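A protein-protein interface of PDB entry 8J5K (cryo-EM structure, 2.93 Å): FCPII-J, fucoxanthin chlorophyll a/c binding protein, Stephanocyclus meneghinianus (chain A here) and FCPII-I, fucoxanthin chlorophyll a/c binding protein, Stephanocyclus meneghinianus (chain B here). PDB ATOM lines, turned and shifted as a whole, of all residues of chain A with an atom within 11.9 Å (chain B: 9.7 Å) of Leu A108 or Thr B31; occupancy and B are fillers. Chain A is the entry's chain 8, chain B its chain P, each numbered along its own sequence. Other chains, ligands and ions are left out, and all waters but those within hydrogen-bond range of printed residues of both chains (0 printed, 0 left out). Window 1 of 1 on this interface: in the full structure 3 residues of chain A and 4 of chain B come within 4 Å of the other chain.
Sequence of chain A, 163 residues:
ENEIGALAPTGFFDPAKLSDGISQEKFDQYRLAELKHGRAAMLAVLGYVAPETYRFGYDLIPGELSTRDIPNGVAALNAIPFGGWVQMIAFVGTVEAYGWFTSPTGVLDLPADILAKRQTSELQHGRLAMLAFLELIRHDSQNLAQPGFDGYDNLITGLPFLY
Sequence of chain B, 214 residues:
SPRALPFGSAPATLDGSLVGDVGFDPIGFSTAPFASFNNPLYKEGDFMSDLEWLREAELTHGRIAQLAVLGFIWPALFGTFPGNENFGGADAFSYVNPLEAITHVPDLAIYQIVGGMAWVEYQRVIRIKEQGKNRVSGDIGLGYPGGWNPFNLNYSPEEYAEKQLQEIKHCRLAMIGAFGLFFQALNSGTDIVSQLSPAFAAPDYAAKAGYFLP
NH2 of Arg A118 lies within hydrogen-bond range of O of Pro B26 (3.3 Å).
The backbone carbonyl oxygen of Gly B28 sits at hydrogen-bond distance from the side-chain hydroxyl of Thr B31 (3.1 Å).
Among the printed residues, pairs that only touch across the chains: Leu A108 with Thr B31, Arg A118 with Ile B27, Leu A108 with Ala B32 and Asp A109 with Thr B31.
No residue of chain B comes within 4 Å of Val A107.
Leu A108 touches two residues of chain B.
Of chain B, only Thr B31 (3.9 Å) comes within 4 Å of Asp A109.
Of the printed residues of chain B, Arg A118 touches Pro B26 and Ile B27.
No residue of chain A comes within 4 Å of Ala B10.
No residue of chain A comes within 4 Å of Pro B11.
No residue of chain A comes within 4 Å of Ala B12.
Of the printed residues of chain A, Pro B26 touches Arg A118 (3.3 Å).
Of the printed residues of chain A, Ile B27 touches Arg A118.
No residue of chain A comes within 4 Å of Gly B28.
No residue of chain A comes within 4 Å of Phe B29.
No residue of chain A comes within 4 Å of Ser B30.
Thr B31 touches two residues of chain A.
Of chain A, only Leu A108 (3.6 Å) comes within 4 Å of Ala B32.
Pro B33 touches none of the printed residues of chain A.
The nearest residue of chain A that does not touch Thr B31 is Leu A110 (5.1 Å).
Of the 21 printed residues of chain B, 4 touch a printed residue of chain A.
Hydrophobic or aromatic side chains of chain B within 4 Å of the printed part of chain A: Ile B27 and Ala B32.
Along chain B the printed residues that touch a printed residue of chain A span positions 26 to 32.
Printed residues of chain A that touch a printed residue of chain B: Leu A108, Asp A109 and Arg A118.
Hydrophobic or aromatic side chains of chain A within 4 Å of the printed part of chain B: Leu A108.
Among the printed residues, 5 pairs touch across the chains.
Among the printed residues, no Asp or Glu carboxylate lies within 4 Å of a Lys or Arg side-chain nitrogen of the other chain.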
ATOM      1  N   THR A 102       7.906  21.727  -4.102  1.00  0.00           N
ATOM      2  CA  THR A 102       7.508  23.133  -3.996  1.00  0.00           C
ATOM      3  C   THR A 102       6.658  23.543  -5.191  1.00  0.00           C
ATOM      4  O   THR A 102       6.880  24.575  -5.826  1.00  0.00           O
ATOM      5  CB  THR A 102       8.723  24.050  -3.855  1.00  0.00           C
ATOM      6  N   SER A 103       5.672  22.703  -5.502  1.00  0.00           N
ATOM      7  CA  SER A 103       4.895  22.751  -6.738  1.00  0.00           C
ATOM      8  C   SER A 103       5.833  22.766  -7.939  1.00  0.00           C
ATOM      9  O   SER A 103       5.946  23.792  -8.631  1.00  0.00           O
ATOM     10  CB  SER A 103       3.970  23.974  -6.750  1.00  0.00           C
ATOM     11  OG  SER A 103       4.697  25.172  -6.910  1.00  0.00           O
ATOM     12  N   PRO A 104       6.512  21.645  -8.213  1.00  0.00           N
ATOM     13  CA  PRO A 104       7.442  21.599  -9.362  1.00  0.00           C
ATOM     14  C   PRO A 104       6.780  21.950 -10.677  1.00  0.00           C
ATOM     15  O   PRO A 104       7.385  22.620 -11.526  1.00  0.00           O
ATOM     16  CB  PRO A 104       7.931  20.144  -9.340  1.00  0.00           C
ATOM     17  N   THR A 105       5.538  21.505 -10.865  1.00  0.00           N
ATOM     18  CA  THR A 105       4.698  21.934 -11.971  1.00  0.00           C
ATOM     19  C   THR A 105       3.311  22.244 -11.424  1.00  0.00           C
ATOM     20  O   THR A 105       3.025  22.045 -10.240  1.00  0.00           O
ATOM     21  CB  THR A 105       4.620  20.871 -13.068  1.00  0.00           C
ATOM     22  N   GLY A 106       2.450  22.754 -12.299  1.00  0.00           N
ATOM     23  CA  GLY A 106       1.072  23.025 -11.941  1.00  0.00           C
ATOM     24  C   GLY A 106       0.849  24.461 -11.519  1.00  0.00           C
ATOM     25  O   GLY A 106       1.282  24.863 -10.437  1.00  0.00           O
ATOM     26  N   VAL A 107       0.221  25.264 -12.376  1.00  0.00           N
ATOM     27  CA  VAL A 107      -0.090  26.642 -12.010  1.00  0.00           C
ATOM     28  C   VAL A 107      -1.503  27.009 -12.446  1.00  0.00           C
ATOM     29  O   VAL A 107      -1.842  28.194 -12.538  1.00  0.00           O
ATOM     30  CB  VAL A 107       0.937  27.620 -12.605  1.00  0.00           C
ATOM     31  N   LEU A 108      -2.321  25.996 -12.744  1.00  0.00           N
ATOM     32  CA  LEU A 108      -3.665  26.142 -13.301  1.00  0.00           C
ATOM     33  C   LEU A 108      -3.652  26.926 -14.610  1.00  0.00           C
ATOM     34  O   LEU A 108      -2.611  27.038 -15.265  1.00  0.00           O
ATOM     35  CB  LEU A 108      -4.601  26.810 -12.292  1.00  0.00           C
ATOM     36  N   ASP A 109      -4.812  27.438 -15.022  1.00  0.00           N
ATOM     37  CA  ASP A 109      -4.906  28.215 -16.253  1.00  0.00           C
ATOM     38  C   ASP A 109      -4.862  29.712 -15.973  1.00  0.00           C
ATOM     39  O   ASP A 109      -3.936  30.397 -16.417  1.00  0.00           O
ATOM     40  CB  ASP A 109      -6.185  27.851 -17.019  1.00  0.00           C
ATOM     41  N   LEU A 110      -5.827  30.222 -15.185  1.00  0.00           N
ATOM     42  CA  LEU A 110      -5.933  31.629 -14.806  1.00  0.00           C
ATOM     43  C   LEU A 110      -5.945  32.536 -16.033  1.00  0.00           C
ATOM     44  O   LEU A 110      -4.881  32.995 -16.463  1.00  0.00           O
ATOM     45  CB  LEU A 110      -4.806  32.029 -13.854  1.00  0.00           C
ATOM     46  N   PRO A 111      -7.117  32.720 -16.693  1.00  0.00           N
ATOM     47  CA  PRO A 111      -7.232  33.679 -17.813  1.00  0.00           C
ATOM     48  C   PRO A 111      -6.538  35.019 -17.574  1.00  0.00           C
ATOM     49  O   PRO A 111      -6.397  35.448 -16.427  1.00  0.00           O
ATOM     50  CB  PRO A 111      -8.750  33.856 -17.957  1.00  0.00           C
ATOM     51  N   ALA A 112      -6.122  35.694 -18.657  1.00  0.00           N
ATOM     52  CA  ALA A 112      -5.122  36.758 -18.556  1.00  0.00           C
ATOM     53  C   ALA A 112      -5.549  37.885 -17.623  1.00  0.00           C
ATOM     54  O   ALA A 112      -4.695  38.519 -16.988  1.00  0.00           O
ATOM     55  CB  ALA A 112      -4.801  37.307 -19.948  1.00  0.00           C
ATOM     56  N   ILE A 114      -7.630  37.644 -14.708  1.00  0.00           N
ATOM     57  CA  ILE A 114      -7.427  37.210 -13.330  1.00  0.00           C
ATOM     58  C   ILE A 114      -5.953  36.919 -13.087  1.00  0.00           C
ATOM     59  O   ILE A 114      -5.439  37.186 -11.998  1.00  0.00           O
ATOM     60  CB  ILE A 114      -8.328  36.000 -12.972  1.00  0.00           C
ATOM     61  CG1 ILE A 114      -8.151  34.847 -13.963  1.00  0.00           C
ATOM     62  CG2 ILE A 114      -9.784  36.419 -12.913  1.00  0.00           C
ATOM     63  CD1 ILE A 114      -9.052  33.656 -13.692  1.00  0.00           C
ATOM     64  N   LEU A 115      -5.247  36.399 -14.096  1.00  0.00           N
ATOM     65  CA  LEU A 115      -3.823  36.106 -13.941  1.00  0.00           C
ATOM     66  C   LEU A 115      -3.026  37.373 -13.663  1.00  0.00           C
ATOM     67  O   LEU A 115      -2.174  37.407 -12.765  1.00  0.00           O
ATOM     68  CB  LEU A 115      -3.295  35.415 -15.199  1.00  0.00           C
ATOM     69  N   ALA A 116      -3.289  38.426 -14.439  1.00  0.00           N
ATOM     70  CA  ALA A 116      -2.599  39.690 -14.222  1.00  0.00           C
ATOM     71  C   ALA A 116      -2.921  40.253 -12.847  1.00  0.00           C
ATOM     72  O   ALA A 116      -2.026  40.731 -12.136  1.00  0.00           O
ATOM     73  CB  ALA A 116      -2.976  40.687 -15.317  1.00  0.00           C
ATOM     74  N   ARG A 118      -3.832  38.635 -10.119  1.00  0.00           N
ATOM     75  CA  ARG A 118      -3.152  37.836  -9.104  1.00  0.00           C
ATOM     76  C   ARG A 118      -1.677  38.190  -9.035  1.00  0.00           C
ATOM     77  O   ARG A 118      -1.112  38.312  -7.943  1.00  0.00           O
ATOM     78  CB  ARG A 118      -3.309  36.339  -9.390  1.00  0.00           C
ATOM     79  CG  ARG A 118      -4.721  35.790  -9.350  1.00  0.00           C
ATOM     80  CD  ARG A 118      -5.337  35.810  -7.973  1.00  0.00           C
ATOM     81  NE  ARG A 118      -6.702  35.299  -8.016  1.00  0.00           N
ATOM     82  CZ  ARG A 118      -7.019  34.012  -8.012  1.00  0.00           C
ATOM     83  NH1 ARG A 118      -6.090  33.071  -7.967  1.00  0.00           N
ATOM     84  NH2 ARG A 118      -8.300  33.659  -8.054  1.00  0.00           N
ATOM     85  N   GLY B   8     -16.522  35.715  -9.968  1.00  0.00           N
ATOM     86  CA  GLY B   8     -16.575  34.757 -11.049  1.00  0.00           C
ATOM     87  C   GLY B   8     -15.769  33.522 -10.703  1.00  0.00           C
ATOM     88  O   GLY B   8     -14.754  33.591 -10.016  1.00  0.00           O
ATOM     89  N   SER B   9     -16.241  32.390 -11.177  1.00  0.00           N
ATOM     90  CA  SER B   9     -15.582  31.128 -10.927  1.00  0.00           C
ATOM     91  C   SER B   9     -14.679  30.793 -12.109  1.00  0.00           C
ATOM     92  O   SER B   9     -14.378  31.646 -12.948  1.00  0.00           O
ATOM     93  CB  SER B   9     -16.626  30.047 -10.651  1.00  0.00           C
ATOM     94  OG  SER B   9     -17.196  30.219  -9.365  1.00  0.00           O
ATOM     95  N   ALA B  10     -14.219  29.548 -12.160  1.00  0.00           N
ATOM     96  CA  ALA B  10     -13.349  29.042 -13.218  1.00  0.00           C
ATOM     97  C   ALA B  10     -13.975  29.272 -14.585  1.00  0.00           C
ATOM     98  O   ALA B  10     -15.208  29.274 -14.701  1.00  0.00           O
ATOM     99  CB  ALA B  10     -13.087  27.549 -13.000  1.00  0.00           C
ATOM    100  N   PRO B  11     -13.175  29.484 -15.639  1.00  0.00           N
ATOM    101  CA  PRO B  11     -13.752  29.638 -16.988  1.00  0.00           C
ATOM    102  C   PRO B  11     -14.533  28.428 -17.439  1.00  0.00           C
ATOM    103  O   PRO B  11     -15.315  28.524 -18.402  1.00  0.00           O
ATOM    104  CB  PRO B  11     -12.515  29.871 -17.879  1.00  0.00           C
ATOM    105  CG  PRO B  11     -11.462  30.365 -16.959  1.00  0.00           C
ATOM    106  CD  PRO B  11     -11.717  29.703 -15.632  1.00  0.00           C
ATOM    107  N   ALA B  12     -14.349  27.288 -16.774  1.00  0.00           N
ATOM    108  CA  ALA B  12     -15.082  26.076 -17.111  1.00  0.00           C
ATOM    109  C   ALA B  12     -15.529  25.267 -15.893  1.00  0.00           C
ATOM    110  O   ALA B  12     -15.717  24.052 -16.016  1.00  0.00           O
ATOM    111  CB  ALA B  12     -14.233  25.181 -18.011  1.00  0.00           C
ATOM    112  N   THR B  13     -15.703  25.875 -14.719  1.00  0.00           N
ATOM    113  CA  THR B  13     -16.284  25.116 -13.621  1.00  0.00           C
ATOM    114  C   THR B  13     -17.714  24.747 -13.985  1.00  0.00           C
ATOM    115  O   THR B  13     -18.433  25.521 -14.622  1.00  0.00           O
ATOM    116  CB  THR B  13     -16.225  25.891 -12.296  1.00  0.00           C
ATOM    117  OG1 THR B  13     -16.598  25.027 -11.213  1.00  0.00           O
ATOM    118  CG2 THR B  13     -17.159  27.064 -12.312  1.00  0.00           C
ATOM    119  N   LEU B  14     -18.102  23.532 -13.648  1.00  0.00           N
ATOM    120  CA  LEU B  14     -19.416  23.075 -14.059  1.00  0.00           C
ATOM    121  C   LEU B  14     -20.416  23.313 -12.936  1.00  0.00           C
ATOM    122  O   LEU B  14     -20.051  23.590 -11.787  1.00  0.00           O
ATOM    123  CB  LEU B  14     -19.366  21.594 -14.460  1.00  0.00           C
ATOM    124  CG  LEU B  14     -20.550  20.969 -15.211  1.00  0.00           C
ATOM    125  CD1 LEU B  14     -21.041  21.893 -16.304  1.00  0.00           C
ATOM    126  CD2 LEU B  14     -20.212  19.600 -15.798  1.00  0.00           C
ATOM    127  N   ASP B  25     -15.383  28.159  -5.882  1.00  0.00           N
ATOM    128  CA  ASP B  25     -14.052  27.727  -6.260  1.00  0.00           C
ATOM    129  C   ASP B  25     -13.211  28.975  -6.499  1.00  0.00           C
ATOM    130  O   ASP B  25     -12.900  29.282  -7.654  1.00  0.00           O
ATOM    131  CB  ASP B  25     -14.103  26.853  -7.512  1.00  0.00           C
ATOM    132  N   PRO B  26     -12.854  29.744  -5.445  1.00  0.00           N
ATOM    133  CA  PRO B  26     -12.172  31.031  -5.664  1.00  0.00           C
ATOM    134  C   PRO B  26     -10.843  30.903  -6.389  1.00  0.00           C
ATOM    135  O   PRO B  26     -10.693  31.426  -7.496  1.00  0.00           O
ATOM    136  CB  PRO B  26     -11.974  31.570  -4.241  1.00  0.00           C
ATOM    137  CG  PRO B  26     -12.994  30.876  -3.427  1.00  0.00           C
ATOM    138  CD  PRO B  26     -13.125  29.509  -4.019  1.00  0.00           C
ATOM    139  N   ILE B  27      -9.876  30.205  -5.791  1.00  0.00           N
ATOM    140  CA  ILE B  27      -8.672  29.883  -6.548  1.00  0.00           C
ATOM    141  C   ILE B  27      -9.007  28.819  -7.575  1.00  0.00           C
ATOM    142  O   ILE B  27      -8.363  28.725  -8.627  1.00  0.00           O
ATOM    143  CB  ILE B  27      -7.534  29.448  -5.611  1.00  0.00           C
ATOM    144  CG1 ILE B  27      -7.391  30.452  -4.474  1.00  0.00           C
ATOM    145  CG2 ILE B  27      -6.213  29.348  -6.362  1.00  0.00           C
ATOM    146  CD1 ILE B  27      -7.008  31.836  -4.939  1.00  0.00           C
ATOM    147  N   GLY B  28     -10.037  28.018  -7.299  1.00  0.00           N
ATOM    148  CA  GLY B  28     -10.606  27.070  -8.238  1.00  0.00           C
ATOM    149  C   GLY B  28      -9.576  26.142  -8.836  1.00  0.00           C
ATOM    150  O   GLY B  28      -9.422  26.099 -10.060  1.00  0.00           O
ATOM    151  N   PHE B  29      -8.872  25.392  -7.986  1.00  0.00           N
ATOM    152  CA  PHE B  29      -7.797  24.519  -8.437  1.00  0.00           C
ATOM    153  C   PHE B  29      -8.285  23.455  -9.405  1.00  0.00           C
ATOM    154  O   PHE B  29      -7.459  22.793 -10.042  1.00  0.00           O
ATOM    155  CB  PHE B  29      -7.112  23.870  -7.232  1.00  0.00           C
ATOM    156  N   SER B  30      -9.595  23.271  -9.507  1.00  0.00           N
ATOM    157  CA  SER B  30     -10.264  22.548 -10.579  1.00  0.00           C
ATOM    158  C   SER B  30      -9.697  22.865 -11.965  1.00  0.00           C
ATOM    159  O   SER B  30      -9.548  21.958 -12.793  1.00  0.00           O
ATOM    160  CB  SER B  30     -11.757  22.875 -10.541  1.00  0.00           C
ATOM    161  OG  SER B  30     -12.429  22.347 -11.663  1.00  0.00           O
ATOM    162  N   THR B  31      -9.393  24.145 -12.223  1.00  0.00           N
ATOM    163  CA  THR B  31      -8.811  24.554 -13.505  1.00  0.00           C
ATOM    164  C   THR B  31      -7.541  23.778 -13.802  1.00  0.00           C
ATOM    165  O   THR B  31      -7.350  23.274 -14.919  1.00  0.00           O
ATOM    166  CB  THR B  31      -8.466  26.043 -13.489  1.00  0.00           C
ATOM    167  OG1 THR B  31      -7.511  26.290 -12.449  1.00  0.00           O
ATOM    168  CG2 THR B  31      -9.684  26.878 -13.262  1.00  0.00           C
ATOM    169  N   ALA B  32      -6.642  23.709 -12.802  1.00  0.00           N
ATOM    170  CA  ALA B  32      -5.364  23.032 -12.917  1.00  0.00           C
ATOM    171  C   ALA B  32      -5.575  21.586 -13.342  1.00  0.00           C
ATOM    172  O   ALA B  32      -6.664  21.034 -13.182  1.00  0.00           O
ATOM    173  CB  ALA B  32      -4.624  23.074 -11.577  1.00  0.00           C
ATOM    174  N   PRO B  33      -4.523  20.949 -13.864  1.00  0.00           N
ATOM    175  CA  PRO B  33      -4.692  19.638 -14.512  1.00  0.00           C
ATOM    176  C   PRO B  33      -5.367  18.619 -13.626  1.00  0.00           C
ATOM    177  O   PRO B  33      -6.157  17.807 -14.129  1.00  0.00           O
ATOM    178  CB  PRO B  33      -3.252  19.230 -14.856  1.00  0.00           C
ATOM    179  N   PHE B  34      -5.097  18.662 -12.313  1.00  0.00           N
ATOM    180  CA  PHE B  34      -5.675  17.759 -11.308  1.00  0.00           C
ATOM    181  C   PHE B  34      -5.581  16.314 -11.771  1.00  0.00           C
ATOM    182  O   PHE B  34      -6.462  15.487 -11.509  1.00  0.00           O
ATOM    183  CB  PHE B  34      -7.116  18.148 -10.970  1.00  0.00           C
ATOM    184  N   ALA B  35      -4.483  15.984 -12.445  1.00  0.00           N
ATOM    185  CA  ALA B  35      -4.304  14.626 -12.966  1.00  0.00           C
ATOM    186  C   ALA B  35      -3.586  13.713 -11.987  1.00  0.00           C
ATOM    187  O   ALA B  35      -3.646  13.933 -10.780  1.00  0.00           O
ATOM    188  CB  ALA B  35      -3.541  14.673 -14.279  1.00  0.00           C
ATOM    189  N   ASP B  50     -10.959  15.296 -13.938  1.00  0.00           N
ATOM    190  CA  ASP B  50     -10.035  15.849 -12.954  1.00  0.00           C
ATOM    191  C   ASP B  50     -10.804  16.520 -11.825  1.00  0.00           C
ATOM    192  O   ASP B  50     -10.463  16.370 -10.640  1.00  0.00           O
ATOM    193  CB  ASP B  50      -9.073  16.825 -13.638  1.00  0.00           C
ATOM    194  CG  ASP B  50      -9.783  18.025 -14.239  1.00  0.00           C
ATOM    195  OD1 ASP B  50     -10.991  17.924 -14.544  1.00  0.00           O
ATOM    196  OD2 ASP B  50      -9.128  19.078 -14.405  1.00  0.00           O
ATOM    197  N   LEU B  51     -11.870  17.236 -12.180  1.00  0.00           N
ATOM    198  CA  LEU B  51     -12.800  17.738 -11.183  1.00  0.00           C
ATOM    199  C   LEU B  51     -13.446  16.596 -10.415  1.00  0.00           C
ATOM    200  O   LEU B  51     -13.556  16.651  -9.190  1.00  0.00           O
ATOM    201  CB  LEU B  51     -13.868  18.589 -11.858  1.00  0.00           C
ATOM    202  CG  LEU B  51     -14.933  19.114 -10.905  1.00  0.00           C
ATOM    203  CD1 LEU B  51     -14.288  19.918  -9.796  1.00  0.00           C
ATOM    204  CD2 LEU B  51     -15.911  19.960 -11.670  1.00  0.00           C
ATOM    205  N   LEU B  54     -11.038  15.350  -7.886  1.00  0.00           N
ATOM    206  CA  LEU B  54     -11.080  16.207  -6.706  1.00  0.00           C
ATOM    207  C   LEU B  54     -12.356  15.977  -5.903  1.00  0.00           C
ATOM    208  O   LEU B  54     -12.364  16.118  -4.672  1.00  0.00           O
ATOM    209  CB  LEU B  54     -10.962  17.666  -7.137  1.00  0.00           C
ATOM    210  CG  LEU B  54     -10.553  18.710  -6.104  1.00  0.00           C
ATOM    211  CD1 LEU B  54      -9.284  18.290  -5.397  1.00  0.00           C
ATOM    212  CD2 LEU B  54     -10.375  20.062  -6.772  1.00  0.00           C
